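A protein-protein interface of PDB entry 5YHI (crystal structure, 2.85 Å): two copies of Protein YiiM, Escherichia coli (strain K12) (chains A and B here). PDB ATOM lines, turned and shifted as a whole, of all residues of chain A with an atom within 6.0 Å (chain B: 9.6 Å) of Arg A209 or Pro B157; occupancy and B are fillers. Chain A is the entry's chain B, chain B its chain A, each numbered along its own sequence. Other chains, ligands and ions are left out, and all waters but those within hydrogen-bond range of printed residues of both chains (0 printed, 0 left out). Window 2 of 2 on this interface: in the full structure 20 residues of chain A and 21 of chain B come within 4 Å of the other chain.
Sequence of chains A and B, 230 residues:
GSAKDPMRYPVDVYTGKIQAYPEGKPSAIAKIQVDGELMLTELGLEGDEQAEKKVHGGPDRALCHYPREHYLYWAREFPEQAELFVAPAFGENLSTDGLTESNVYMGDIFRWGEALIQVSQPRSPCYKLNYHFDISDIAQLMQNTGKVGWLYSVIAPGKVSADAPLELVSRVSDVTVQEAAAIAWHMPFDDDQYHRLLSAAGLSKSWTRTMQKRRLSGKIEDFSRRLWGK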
ATOM      1  N   LEU A 198     -31.520  17.513 -26.371  1.00  0.00           N
ATOM      2  CA  LEU A 198     -30.749  16.284 -26.055  1.00  0.00           C
ATOM      3  C   LEU A 198     -30.225  15.543 -27.286  1.00  0.00           C
ATOM      4  O   LEU A 198     -29.254  14.839 -27.187  1.00  0.00           O
ATOM      5  CB  LEU A 198     -31.576  15.333 -25.184  1.00  0.00           C
ATOM      6  CG  LEU A 198     -31.795  15.810 -23.743  1.00  0.00           C
ATOM      7  CD1 LEU A 198     -32.872  14.971 -23.083  1.00  0.00           C
ATOM      8  CD2 LEU A 198     -30.525  15.749 -22.953  1.00  0.00           C
ATOM      9  N   SER A 204     -22.881  19.662 -24.178  1.00  0.00           N
ATOM     10  CA  SER A 204     -22.109  19.453 -22.970  1.00  0.00           C
ATOM     11  C   SER A 204     -22.818  18.507 -22.022  1.00  0.00           C
ATOM     12  O   SER A 204     -24.035  18.362 -22.040  1.00  0.00           O
ATOM     13  CB  SER A 204     -21.858  20.790 -22.257  1.00  0.00           C
ATOM     14  OG  SER A 204     -23.054  21.301 -21.710  1.00  0.00           O
ATOM     15  N   LYS A 205     -22.020  17.882 -21.177  1.00  0.00           N
ATOM     16  CA  LYS A 205     -22.500  17.001 -20.135  1.00  0.00           C
ATOM     17  C   LYS A 205     -23.486  17.698 -19.192  1.00  0.00           C
ATOM     18  O   LYS A 205     -24.541  17.153 -18.882  1.00  0.00           O
ATOM     19  CB  LYS A 205     -21.293  16.499 -19.366  1.00  0.00           C
ATOM     20  CG  LYS A 205     -21.536  15.374 -18.418  1.00  0.00           C
ATOM     21  CD  LYS A 205     -20.197  14.898 -17.870  1.00  0.00           C
ATOM     22  CE  LYS A 205     -20.002  13.439 -18.039  1.00  0.00           C
ATOM     23  NZ  LYS A 205     -18.627  13.061 -17.675  1.00  0.00           N
ATOM     24  N   SER A 206     -23.158  18.906 -18.746  1.00  0.00           N
ATOM     25  CA  SER A 206     -24.044  19.593 -17.803  1.00  0.00           C
ATOM     26  C   SER A 206     -25.387  19.967 -18.412  1.00  0.00           C
ATOM     27  O   SER A 206     -26.410  19.914 -17.726  1.00  0.00           O
ATOM     28  CB  SER A 206     -23.388  20.836 -17.201  1.00  0.00           C
ATOM     29  OG  SER A 206     -22.897  21.672 -18.215  1.00  0.00           O
ATOM     30  N   TRP A 207     -25.395  20.348 -19.684  1.00  0.00           N
ATOM     31  CA  TRP A 207     -26.667  20.685 -20.337  1.00  0.00           C
ATOM     32  C   TRP A 207     -27.477  19.421 -20.569  1.00  0.00           C
ATOM     33  O   TRP A 207     -28.668  19.429 -20.337  1.00  0.00           O
ATOM     34  CB  TRP A 207     -26.449  21.488 -21.620  1.00  0.00           C
ATOM     35  CG  TRP A 207     -26.229  22.937 -21.306  1.00  0.00           C
ATOM     36  CD1 TRP A 207     -25.328  23.449 -20.430  1.00  0.00           C
ATOM     37  CD2 TRP A 207     -26.954  24.054 -21.823  1.00  0.00           C
ATOM     38  NE1 TRP A 207     -25.444  24.808 -20.370  1.00  0.00           N
ATOM     39  CE2 TRP A 207     -26.442  25.204 -21.213  1.00  0.00           C
ATOM     40  CE3 TRP A 207     -27.987  24.191 -22.741  1.00  0.00           C
ATOM     41  CZ2 TRP A 207     -26.916  26.462 -21.499  1.00  0.00           C
ATOM     42  CZ3 TRP A 207     -28.461  25.448 -23.014  1.00  0.00           C
ATOM     43  CH2 TRP A 207     -27.922  26.563 -22.407  1.00  0.00           C
ATOM     44  N   THR A 208     -26.815  18.323 -20.942  1.00  0.00           N
ATOM     45  CA  THR A 208     -27.461  17.030 -21.038  1.00  0.00           C
ATOM     46  C   THR A 208     -28.078  16.658 -19.690  1.00  0.00           C
ATOM     47  O   THR A 208     -29.228  16.241 -19.638  1.00  0.00           O
ATOM     48  CB  THR A 208     -26.467  15.911 -21.464  1.00  0.00           C
ATOM     49  OG1 THR A 208     -25.823  16.254 -22.700  1.00  0.00           O
ATOM     50  CG2 THR A 208     -27.184  14.565 -21.585  1.00  0.00           C
ATOM     51  N   ARG A 209     -27.321  16.810 -18.605  1.00  0.00           N
ATOM     52  CA  ARG A 209     -27.828  16.487 -17.276  1.00  0.00           C
ATOM     53  C   ARG A 209     -29.002  17.373 -16.919  1.00  0.00           C
ATOM     54  O   ARG A 209     -30.040  16.880 -16.464  1.00  0.00           O
ATOM     55  CB  ARG A 209     -26.742  16.635 -16.235  1.00  0.00           C
ATOM     56  CG  ARG A 209     -27.187  16.428 -14.782  1.00  0.00           C
ATOM     57  CD  ARG A 209     -25.972  16.343 -13.830  1.00  0.00           C
ATOM     58  NE  ARG A 209     -24.860  17.156 -14.336  1.00  0.00           N
ATOM     59  CZ  ARG A 209     -23.550  16.936 -14.141  1.00  0.00           C
ATOM     60  NH1 ARG A 209     -23.098  15.909 -13.419  1.00  0.00           N
ATOM     61  NH2 ARG A 209     -22.668  17.773 -14.687  1.00  0.00           N
ATOM     62  N   THR A 210     -28.854  18.676 -17.160  1.00  0.00           N
ATOM     63  CA  THR A 210     -29.909  19.633 -16.854  1.00  0.00           C
ATOM     64  C   THR A 210     -31.218  19.280 -17.584  1.00  0.00           C
ATOM     65  O   THR A 210     -32.288  19.209 -16.965  1.00  0.00           O
ATOM     66  CB  THR A 210     -29.462  21.068 -17.185  1.00  0.00           C
ATOM     67  OG1 THR A 210     -28.468  21.457 -16.251  1.00  0.00           O
ATOM     68  CG2 THR A 210     -30.589  22.071 -17.071  1.00  0.00           C
ATOM     69  N   MET A 211     -31.124  19.055 -18.889  1.00  0.00           N
ATOM     70  CA  MET A 211     -32.306  18.870 -19.714  1.00  0.00           C
ATOM     71  C   MET A 211     -32.939  17.528 -19.437  1.00  0.00           C
ATOM     72  O   MET A 211     -34.172  17.393 -19.450  1.00  0.00           O
ATOM     73  CB  MET A 211     -31.968  18.971 -21.199  1.00  0.00           C
ATOM     74  CG  MET A 211     -31.451  20.338 -21.628  1.00  0.00           C
ATOM     75  SD  MET A 211     -32.681  21.625 -21.454  1.00  0.00           S
ATOM     76  CE  MET A 211     -31.679  23.045 -21.187  1.00  0.00           C
ATOM     77  N   GLN A 212     -32.114  16.523 -19.191  1.00  0.00           N
ATOM     78  CA  GLN A 212     -32.668  15.223 -18.878  1.00  0.00           C
ATOM     79  C   GLN A 212     -33.461  15.323 -17.579  1.00  0.00           C
ATOM     80  O   GLN A 212     -34.541  14.734 -17.454  1.00  0.00           O
ATOM     81  CB  GLN A 212     -31.586  14.137 -18.776  1.00  0.00           C
ATOM     82  CG  GLN A 212     -32.158  12.747 -18.428  1.00  0.00           C
ATOM     83  CD  GLN A 212     -33.142  12.225 -19.471  1.00  0.00           C
ATOM     84  OE1 GLN A 212     -32.742  11.849 -20.562  1.00  0.00           O
ATOM     85  NE2 GLN A 212     -34.428  12.190 -19.133  1.00  0.00           N
ATOM     86  N   LYS A 213     -32.927  16.079 -16.621  1.00  0.00           N
ATOM     87  CA  LYS A 213     -33.562  16.183 -15.320  1.00  0.00           C
ATOM     88  C   LYS A 213     -34.896  16.869 -15.419  1.00  0.00           C
ATOM     89  O   LYS A 213     -35.805  16.526 -14.669  1.00  0.00           O
ATOM     90  CB  LYS A 213     -32.678  16.914 -14.318  1.00  0.00           C
ATOM     91  CG  LYS A 213     -31.560  16.064 -13.741  1.00  0.00           C
ATOM     92  CD  LYS A 213     -31.044  16.626 -12.410  1.00  0.00           C
ATOM     93  CE  LYS A 213     -29.888  15.756 -11.873  1.00  0.00           C
ATOM     94  NZ  LYS A 213     -30.326  14.495 -11.184  1.00  0.00           N
ATOM     95  N   ARG A 214     -35.012  17.836 -16.332  1.00  0.00           N
ATOM     96  CA  ARG A 214     -36.294  18.507 -16.584  1.00  0.00           C
ATOM     97  C   ARG A 214     -37.323  17.456 -17.044  1.00  0.00           C
ATOM     98  O   ARG A 214     -38.441  17.376 -16.528  1.00  0.00           O
ATOM     99  CB  ARG A 214     -36.152  19.620 -17.639  1.00  0.00           C
ATOM    100  CG  ARG A 214     -35.252  20.778 -17.241  1.00  0.00           C
ATOM    101  CD  ARG A 214     -35.476  21.991 -18.151  1.00  0.00           C
ATOM    102  NE  ARG A 214     -34.561  23.111 -17.876  1.00  0.00           N
ATOM    103  CZ  ARG A 214     -34.551  24.276 -18.540  1.00  0.00           C
ATOM    104  NH1 ARG A 214     -35.406  24.502 -19.536  1.00  0.00           N
ATOM    105  NH2 ARG A 214     -33.689  25.232 -18.207  1.00  0.00           N
ATOM    106  N   LEU B  38     -23.518   0.442  -4.399  1.00  0.00           N
ATOM    107  CA  LEU B  38     -22.241   1.129  -4.588  1.00  0.00           C
ATOM    108  C   LEU B  38     -22.398   2.458  -5.349  1.00  0.00           C
ATOM    109  O   LEU B  38     -23.472   2.764  -5.850  1.00  0.00           O
ATOM    110  CB  LEU B  38     -21.218   0.183  -5.249  1.00  0.00           C
ATOM    111  CG  LEU B  38     -21.343  -0.137  -6.741  1.00  0.00           C
ATOM    112  CD1 LEU B  38     -20.279  -1.167  -7.177  1.00  0.00           C
ATOM    113  CD2 LEU B  38     -22.747  -0.618  -7.075  1.00  0.00           C
ATOM    114  N   MET B  39     -21.325   3.245  -5.410  1.00  0.00           N
ATOM    115  CA  MET B  39     -21.380   4.616  -5.950  1.00  0.00           C
ATOM    116  C   MET B  39     -20.785   4.725  -7.355  1.00  0.00           C
ATOM    117  O   MET B  39     -19.638   4.332  -7.584  1.00  0.00           O
ATOM    118  CB  MET B  39     -20.653   5.587  -5.005  1.00  0.00           C
ATOM    119  CG  MET B  39     -20.817   7.085  -5.338  1.00  0.00           C
ATOM    120  SD  MET B  39     -22.517   7.744  -5.262  1.00  0.00           S
ATOM    121  CE  MET B  39     -22.189   9.381  -4.565  1.00  0.00           C
ATOM    122  N   LEU B  40     -21.572   5.261  -8.287  1.00  0.00           N
ATOM    123  CA  LEU B  40     -21.095   5.545  -9.637  1.00  0.00           C
ATOM    124  C   LEU B  40     -20.662   6.987  -9.705  1.00  0.00           C
ATOM    125  O   LEU B  40     -21.506   7.887  -9.684  1.00  0.00           O
ATOM    126  CB  LEU B  40     -22.179   5.298 -10.689  1.00  0.00           C
ATOM    127  CG  LEU B  40     -21.761   5.480 -12.158  1.00  0.00           C
ATOM    128  CD1 LEU B  40     -20.812   4.383 -12.598  1.00  0.00           C
ATOM    129  CD2 LEU B  40     -22.978   5.490 -13.051  1.00  0.00           C
ATOM    130  N   THR B  41     -19.349   7.195  -9.791  1.00  0.00           N
ATOM    131  CA  THR B  41     -18.780   8.531  -9.897  1.00  0.00           C
ATOM    132  C   THR B  41     -18.654   8.933 -11.354  1.00  0.00           C
ATOM    133  O   THR B  41     -18.824   8.125 -12.249  1.00  0.00           O
ATOM    134  CB  THR B  41     -17.386   8.609  -9.256  1.00  0.00           C
ATOM    135  OG1 THR B  41     -16.452   7.879 -10.060  1.00  0.00           O
ATOM    136  CG2 THR B  41     -17.402   8.060  -7.819  1.00  0.00           C
ATOM    137  N   GLU B  42     -18.360  10.202 -11.575  1.00  0.00           N
ATOM    138  CA  GLU B  42     -18.057  10.735 -12.901  1.00  0.00           C
ATOM    139  C   GLU B  42     -17.001   9.853 -13.603  1.00  0.00           C
ATOM    140  O   GLU B  42     -17.085   9.656 -14.811  1.00  0.00           O
ATOM    141  CB  GLU B  42     -17.557  12.206 -12.765  1.00  0.00           C
ATOM    142  CG  GLU B  42     -18.130  13.252 -13.764  1.00  0.00           C
ATOM    143  CD  GLU B  42     -19.636  13.507 -13.584  1.00  0.00           C
ATOM    144  OE1 GLU B  42     -20.036  14.623 -13.156  1.00  0.00           O
ATOM    145  OE2 GLU B  42     -20.424  12.583 -13.875  1.00  0.00           O
ATOM    146  N   LEU B  43     -16.038   9.305 -12.847  1.00  0.00           N
ATOM    147  CA  LEU B  43     -14.919   8.520 -13.410  1.00  0.00           C
ATOM    148  C   LEU B  43     -15.090   6.975 -13.420  1.00  0.00           C
ATOM    149  O   LEU B  43     -14.139   6.248 -13.728  1.00  0.00           O
ATOM    150  CB  LEU B  43     -13.624   8.882 -12.675  1.00  0.00           C
ATOM    151  CG  LEU B  43     -12.794   9.957 -13.386  1.00  0.00           C
ATOM    152  CD1 LEU B  43     -11.739  10.594 -12.469  1.00  0.00           C
ATOM    153  CD2 LEU B  43     -12.144   9.342 -14.634  1.00  0.00           C
ATOM    154  N   GLY B  44     -16.288   6.483 -13.102  1.00  0.00           N
ATOM    155  CA  GLY B  44     -16.544   5.050 -12.981  1.00  0.00           C
ATOM    156  C   GLY B  44     -17.074   4.667 -11.614  1.00  0.00           C
ATOM    157  O   GLY B  44     -17.250   5.525 -10.747  1.00  0.00           O
ATOM    158  N   LEU B  45     -17.328   3.378 -11.416  1.00  0.00           N
ATOM    159  CA  LEU B  45     -17.763   2.879 -10.114  1.00  0.00           C
ATOM    160  C   LEU B  45     -16.605   2.887  -9.104  1.00  0.00           C
ATOM    161  O   LEU B  45     -15.435   2.800  -9.495  1.00  0.00           O
ATOM    162  CB  LEU B  45     -18.320   1.462 -10.260  1.00  0.00           C
ATOM    163  CG  LEU B  45     -19.584   1.256 -11.111  1.00  0.00           C
ATOM    164  CD1 LEU B  45     -19.577  -0.124 -11.735  1.00  0.00           C
ATOM    165  CD2 LEU B  45     -20.858   1.500 -10.283  1.00  0.00           C
ATOM    166  N   ILE B 109     -29.856   7.514 -23.290  1.00  0.00           N
ATOM    167  CA  ILE B 109     -29.683   7.806 -21.863  1.00  0.00           C
ATOM    168  C   ILE B 109     -30.521   6.824 -21.043  1.00  0.00           C
ATOM    169  O   ILE B 109     -31.731   6.646 -21.292  1.00  0.00           O
ATOM    170  CB  ILE B 109     -30.087   9.245 -21.511  1.00  0.00           C
ATOM    171  CG1 ILE B 109     -29.230  10.256 -22.298  1.00  0.00           C
ATOM    172  CG2 ILE B 109     -29.938   9.470 -20.029  1.00  0.00           C
ATOM    173  CD1 ILE B 109     -29.663  11.677 -22.155  1.00  0.00           C
ATOM    174  N   TRP B 112     -30.094   4.519 -14.033  1.00  0.00           N
ATOM    175  CA  TRP B 112     -29.683   3.350 -13.283  1.00  0.00           C
ATOM    176  C   TRP B 112     -29.643   3.716 -11.808  1.00  0.00           C
ATOM    177  O   TRP B 112     -28.754   4.431 -11.366  1.00  0.00           O
ATOM    178  CB  TRP B 112     -28.313   2.873 -13.736  1.00  0.00           C
ATOM    179  CG  TRP B 112     -27.881   1.638 -13.056  1.00  0.00           C
ATOM    180  CD1 TRP B 112     -28.691   0.662 -12.528  1.00  0.00           C
ATOM    181  CD2 TRP B 112     -26.547   1.191 -12.863  1.00  0.00           C
ATOM    182  NE1 TRP B 112     -27.937  -0.352 -11.999  1.00  0.00           N
ATOM    183  CE2 TRP B 112     -26.612  -0.049 -12.189  1.00  0.00           C
ATOM    184  CE3 TRP B 112     -25.301   1.706 -13.195  1.00  0.00           C
ATOM    185  CZ2 TRP B 112     -25.463  -0.772 -11.834  1.00  0.00           C
ATOM    186  CZ3 TRP B 112     -24.166   0.994 -12.836  1.00  0.00           C
ATOM    187  CH2 TRP B 112     -24.254  -0.231 -12.170  1.00  0.00           C
ATOM    188  N   GLY B 113     -30.611   3.225 -11.048  1.00  0.00           N
ATOM    189  CA  GLY B 113     -30.769   3.641  -9.665  1.00  0.00           C
ATOM    190  C   GLY B 113     -30.943   5.132  -9.639  1.00  0.00           C
ATOM    191  O   GLY B 113     -31.924   5.647 -10.169  1.00  0.00           O
ATOM    192  N   GLU B 114     -29.958   5.818  -9.060  1.00  0.00           N
ATOM    193  CA  GLU B 114     -29.989   7.282  -8.889  1.00  0.00           C
ATOM    194  C   GLU B 114     -29.207   8.021  -9.978  1.00  0.00           C
ATOM    195  O   GLU B 114     -29.274   9.249 -10.061  1.00  0.00           O
ATOM    196  CB  GLU B 114     -29.395   7.677  -7.527  1.00  0.00           C
ATOM    197  CG  GLU B 114     -30.319   7.533  -6.309  1.00  0.00           C
ATOM    198  CD  GLU B 114     -29.701   8.178  -5.040  1.00  0.00           C
ATOM    199  OE1 GLU B 114     -30.446   8.418  -4.057  1.00  0.00           O
ATOM    200  OE2 GLU B 114     -28.470   8.460  -5.036  1.00  0.00           O
ATOM    201  N   ALA B 115     -28.464   7.286 -10.796  1.00  0.00           N
ATOM    202  CA  ALA B 115     -27.552   7.890 -11.747  1.00  0.00           C
ATOM    203  C   ALA B 115     -28.154   7.908 -13.153  1.00  0.00           C
ATOM    204  O   ALA B 115     -29.145   7.223 -13.437  1.00  0.00           O
ATOM    205  CB  ALA B 115     -26.219   7.144 -11.741  1.00  0.00           C
ATOM    206  N   LEU B 116     -27.543   8.724 -14.012  1.00  0.00           N
ATOM    207  CA  LEU B 116     -27.859   8.783 -15.430  1.00  0.00           C
ATOM    208  C   LEU B 116     -26.605   8.465 -16.247  1.00  0.00           C
ATOM    209  O   LEU B 116     -25.521   8.936 -15.937  1.00  0.00           O
ATOM    210  CB  LEU B 116     -28.360  10.181 -15.801  1.00  0.00           C
ATOM    211  CG  LEU B 116     -29.687  10.616 -15.210  1.00  0.00           C
ATOM    212  CD1 LEU B 116     -29.912  12.014 -15.649  1.00  0.00           C
ATOM    213  CD2 LEU B 116     -30.820   9.739 -15.666  1.00  0.00           C
ATOM    214  N   ILE B 117     -26.747   7.673 -17.293  1.00  0.00           N
ATOM    215  CA  ILE B 117     -25.609   7.330 -18.140  1.00  0.00           C
ATOM    216  C   ILE B 117     -26.013   7.386 -19.615  1.00  0.00           C
ATOM    217  O   ILE B 117     -27.184   7.184 -19.954  1.00  0.00           O
ATOM    218  CB  ILE B 117     -25.025   5.927 -17.775  1.00  0.00           C
ATOM    219  CG1 ILE B 117     -25.993   4.797 -18.133  1.00  0.00           C
ATOM    220  CG2 ILE B 117     -24.721   5.846 -16.283  1.00  0.00           C
ATOM    221  CD1 ILE B 117     -25.642   3.473 -17.473  1.00  0.00           C
ATOM    222  N   GLN B 118     -25.051   7.667 -20.485  1.00  0.00           N
ATOM    223  CA  GLN B 118     -25.322   7.865 -21.903  1.00  0.00           C
ATOM    224  C   GLN B 118     -24.370   7.019 -22.723  1.00  0.00           C
ATOM    225  O   GLN B 118     -23.202   6.906 -22.368  1.00  0.00           O
ATOM    226  CB  GLN B 118     -25.180   9.349 -22.277  1.00  0.00           C
ATOM    227  CG  GLN B 118     -25.717   9.709 -23.653  1.00  0.00           C
ATOM    228  CD  GLN B 118     -25.522  11.166 -23.995  1.00  0.00           C
ATOM    229  OE1 GLN B 118     -24.450  11.726 -23.799  1.00  0.00           O
ATOM    230  NE2 GLN B 118     -26.558  11.795 -24.503  1.00  0.00           N
ATOM    231  N   SER B 153     -20.792   7.361 -20.797  1.00  0.00           N
ATOM    232  CA  SER B 153     -20.310   8.489 -19.991  1.00  0.00           C
ATOM    233  C   SER B 153     -21.338   8.729 -18.901  1.00  0.00           C
ATOM    234  O   SER B 153     -22.516   8.511 -19.120  1.00  0.00           O
ATOM    235  CB  SER B 153     -20.159   9.741 -20.833  1.00  0.00           C
ATOM    236  OG  SER B 153     -21.394  10.408 -20.899  1.00  0.00           O
ATOM    237  N   VAL B 154     -20.893   9.171 -17.732  1.00  0.00           N
ATOM    238  CA  VAL B 154     -21.780   9.308 -16.598  1.00  0.00           C
ATOM    239  C   VAL B 154     -22.292  10.739 -16.566  1.00  0.00           C
ATOM    240  O   VAL B 154     -21.528  11.673 -16.349  1.00  0.00           O
ATOM    241  CB  VAL B 154     -21.085   8.931 -15.287  1.00  0.00           C
ATOM    242  CG1 VAL B 154     -22.018   9.155 -14.091  1.00  0.00           C
ATOM    243  CG2 VAL B 154     -20.628   7.483 -15.345  1.00  0.00           C
ATOM    244  N   ILE B 155     -23.595  10.898 -16.790  1.00  0.00           N
ATOM    245  CA  ILE B 155     -24.229  12.206 -16.898  1.00  0.00           C
ATOM    246  C   ILE B 155     -24.549  12.757 -15.499  1.00  0.00           C
ATOM    247  O   ILE B 155     -24.349  13.935 -15.225  1.00  0.00           O
ATOM    248  CB  ILE B 155     -25.496  12.129 -17.788  1.00  0.00           C
ATOM    249  CG1 ILE B 155     -25.132  11.642 -19.206  1.00  0.00           C
ATOM    250  CG2 ILE B 155     -26.194  13.462 -17.865  1.00  0.00           C
ATOM    251  CD1 ILE B 155     -24.041  12.411 -19.919  1.00  0.00           C
ATOM    252  N   ALA B 156     -25.026  11.898 -14.611  1.00  0.00           N
ATOM    253  CA  ALA B 156     -25.223  12.272 -13.225  1.00  0.00           C
ATOM    254  C   ALA B 156     -24.678  11.157 -12.331  1.00  0.00           C
ATOM    255  O   ALA B 156     -25.123  10.010 -12.455  1.00  0.00           O
ATOM    256  CB  ALA B 156     -26.685  12.493 -12.963  1.00  0.00           C
ATOM    257  N   PRO B 157     -23.736  11.478 -11.418  1.00  0.00           N
ATOM    258  CA  PRO B 157     -23.261  10.501 -10.445  1.00  0.00           C
ATOM    259  C   PRO B 157     -24.334  10.172  -9.409  1.00  0.00           C
ATOM    260  O   PRO B 157     -25.132  11.042  -9.060  1.00  0.00           O
ATOM    261  CB  PRO B 157     -22.108  11.224  -9.741  1.00  0.00           C
ATOM    262  CG  PRO B 157     -21.967  12.552 -10.389  1.00  0.00           C
ATOM    263  CD  PRO B 157     -23.277  12.823 -11.064  1.00  0.00           C
ATOM    264  N   GLY B 158     -24.351   8.935  -8.918  1.00  0.00           N
ATOM    265  CA  GLY B 158     -25.365   8.531  -7.945  1.00  0.00           C
ATOM    266  C   GLY B 158     -25.214   7.136  -7.381  1.00  0.00           C
ATOM    267  O   GLY B 158     -24.358   6.379  -7.825  1.00  0.00           O
ATOM    268  N   LYS B 159     -26.040   6.813  -6.381  1.00  0.00           N
ATOM    269  CA  LYS B 159     -26.054   5.484  -5.765  1.00  0.00           C
ATOM    270  C   LYS B 159     -26.675   4.493  -6.745  1.00  0.00           C
ATOM    271  O   LYS B 159     -27.785   4.719  -7.246  1.00  0.00           O
ATOM    272  CB  LYS B 159     -26.841   5.481  -4.441  1.00  0.00           C
ATOM    273  CG  LYS B 159     -26.079   6.010  -3.205  1.00  0.00           C
ATOM    274  N   VAL B 160     -25.946   3.409  -7.014  1.00  0.00           N
ATOM    275  CA  VAL B 160     -26.382   2.357  -7.938  1.00  0.00           C
ATOM    276  C   VAL B 160     -26.330   1.000  -7.240  1.00  0.00           C
ATOM    277  O   VAL B 160     -25.822   0.899  -6.126  1.00  0.00           O
ATOM    278  CB  VAL B 160     -25.499   2.326  -9.214  1.00  0.00           C
ATOM    279  CG1 VAL B 160     -25.696   3.584 -10.015  1.00  0.00           C
ATOM    280  CG2 VAL B 160     -24.025   2.167  -8.855  1.00  0.00           C
ATOM    281  N   VAL B 169     -34.444   6.194 -20.658  1.00  0.00           N
ATOM    282  CA  VAL B 169     -35.287   7.368 -20.451  1.00  0.00           C
ATOM    283  C   VAL B 169     -35.271   8.326 -21.633  1.00  0.00           C
ATOM    284  O   VAL B 169     -36.248   9.012 -21.845  1.00  0.00           O
ATOM    285  CB  VAL B 169     -34.979   8.119 -19.122  1.00  0.00           C
ATOM    286  CG1 VAL B 169     -35.103   7.146 -17.953  1.00  0.00           C
ATOM    287  CG2 VAL B 169     -33.605   8.821 -19.146  1.00  0.00           C
ATOM    288  N   SER B 170     -34.197   8.374 -22.405  1.00  0.00           N
ATOM    289  CA  SER B 170     -34.195   9.169 -23.627  1.00  0.00           C
ATOM    290  C   SER B 170     -33.478   8.460 -24.741  1.00  0.00           C
ATOM    291  O   SER B 170     -32.353   8.004 -24.547  1.00  0.00           O
ATOM    292  CB  SER B 170     -33.496  10.500 -23.404  1.00  0.00           C
ATOM    293  OG  SER B 170     -34.352  11.364 -22.733  1.00  0.00           O
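NH1 of Arg A209 lies within salt-bridge range of OE1 of Glu B42 (3.3 Å). The side-chain hydroxyl (OG) of Ser B170 is in hydrogen-bond range of the side-chain amide oxygen (OE1) of Gln A212 (2.7 Å). The backbone carbonyl oxygen (O) of Val B154 lies close to the side-chain amino group (NZ) of Lys A205 (3.5 Å). NH1 of Arg A209 is in hydrogen-bond range of O of Ile B155, at 3.0 Å.
OG of Ser B170 touches CD1 of Leu A198 (3.9 Å). Lys A205 touches Glu B42 (NZ to CG, 3.9 Å). Ile B109 touches Thr A208 (CD1 to CG2, 3.8 Å). Arg A209 touches Pro B157 (NH1 to CD, 3.9 Å). Gln A212 touches Ile B109. Gln A212 touches Leu B116 (CG to CD1, 3.6 Å). CG2 of Val B169 touches CD of Gln A212, 3.5 Å away.
O of Leu B116 sits at hydrogen-bond distance from N of Ile B155, at 2.9 Å. N of Val B169 lies within hydrogen-bond range of O of Ile B109, 2.8 Å away. The side-chain hydroxyl of Thr A208 sits at hydrogen-bond distance from the backbone carbonyl oxygen of Ser A204, at 2.8 Å. O of Ala B156 sits at hydrogen-bond distance from N of Leu B116 (3.2 Å). The backbone NH (N) of Ile B109 is in hydrogen-bond range of the backbone carbonyl oxygen (O) of Ser B170, at 2.8 Å.
No position is printed for both chains. Of the 11 pairs that touch across the chains among the printed residues, none has its exchanged pair printed and touching as well.
Of the 26 printed residues of chain B, 8 touch a printed residue of chain A. Printed residues of chain B that touch a printed residue of chain A: Glu B42, Ile B109, Leu B116, Val B154, Ile B155, Pro B157, Val B169 and Ser B170. Hydrophobic or aromatic side chains of chain B that line the printed part of chain A: Ile B109, Leu B116, Ile B155, Pro B157 and Val B169. Of the 12 printed residues of chain A, 5 touch a printed residue of chain B. Hydrophobic or aromatic side chains of chain A that line the printed part of chain B: Leu A198. Among the printed residues, Asp or Glu carboxylates within 4 Å of a Lys or Arg side-chain nitrogen of the other chain: Arg A209 with Glu B42.
Printed residues of chain B within 4 Å of Arg A209: Glu B42, Ile B155 and Pro B157. Of the printed residues of chain A, Pro B157 touches Arg A209. No residue of chain B comes within 4 Å of Ser A206. No residue of chain B comes within 4 Å of Thr A210. Printed residues of chain A within 4 Å of Leu B116: Gln A212 (3.6 Å). Printed residues of chain B within 4 Å of Thr A208: Ile B109 (3.8 Å). Of the printed residues of chain A, Ile B109 touches Thr A208 (3.8 Å) and Gln A212 (3.5 Å). Ala B115 touches none of the printed residues of chain A. Leu B45 touches none of the printed residues of chain A.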
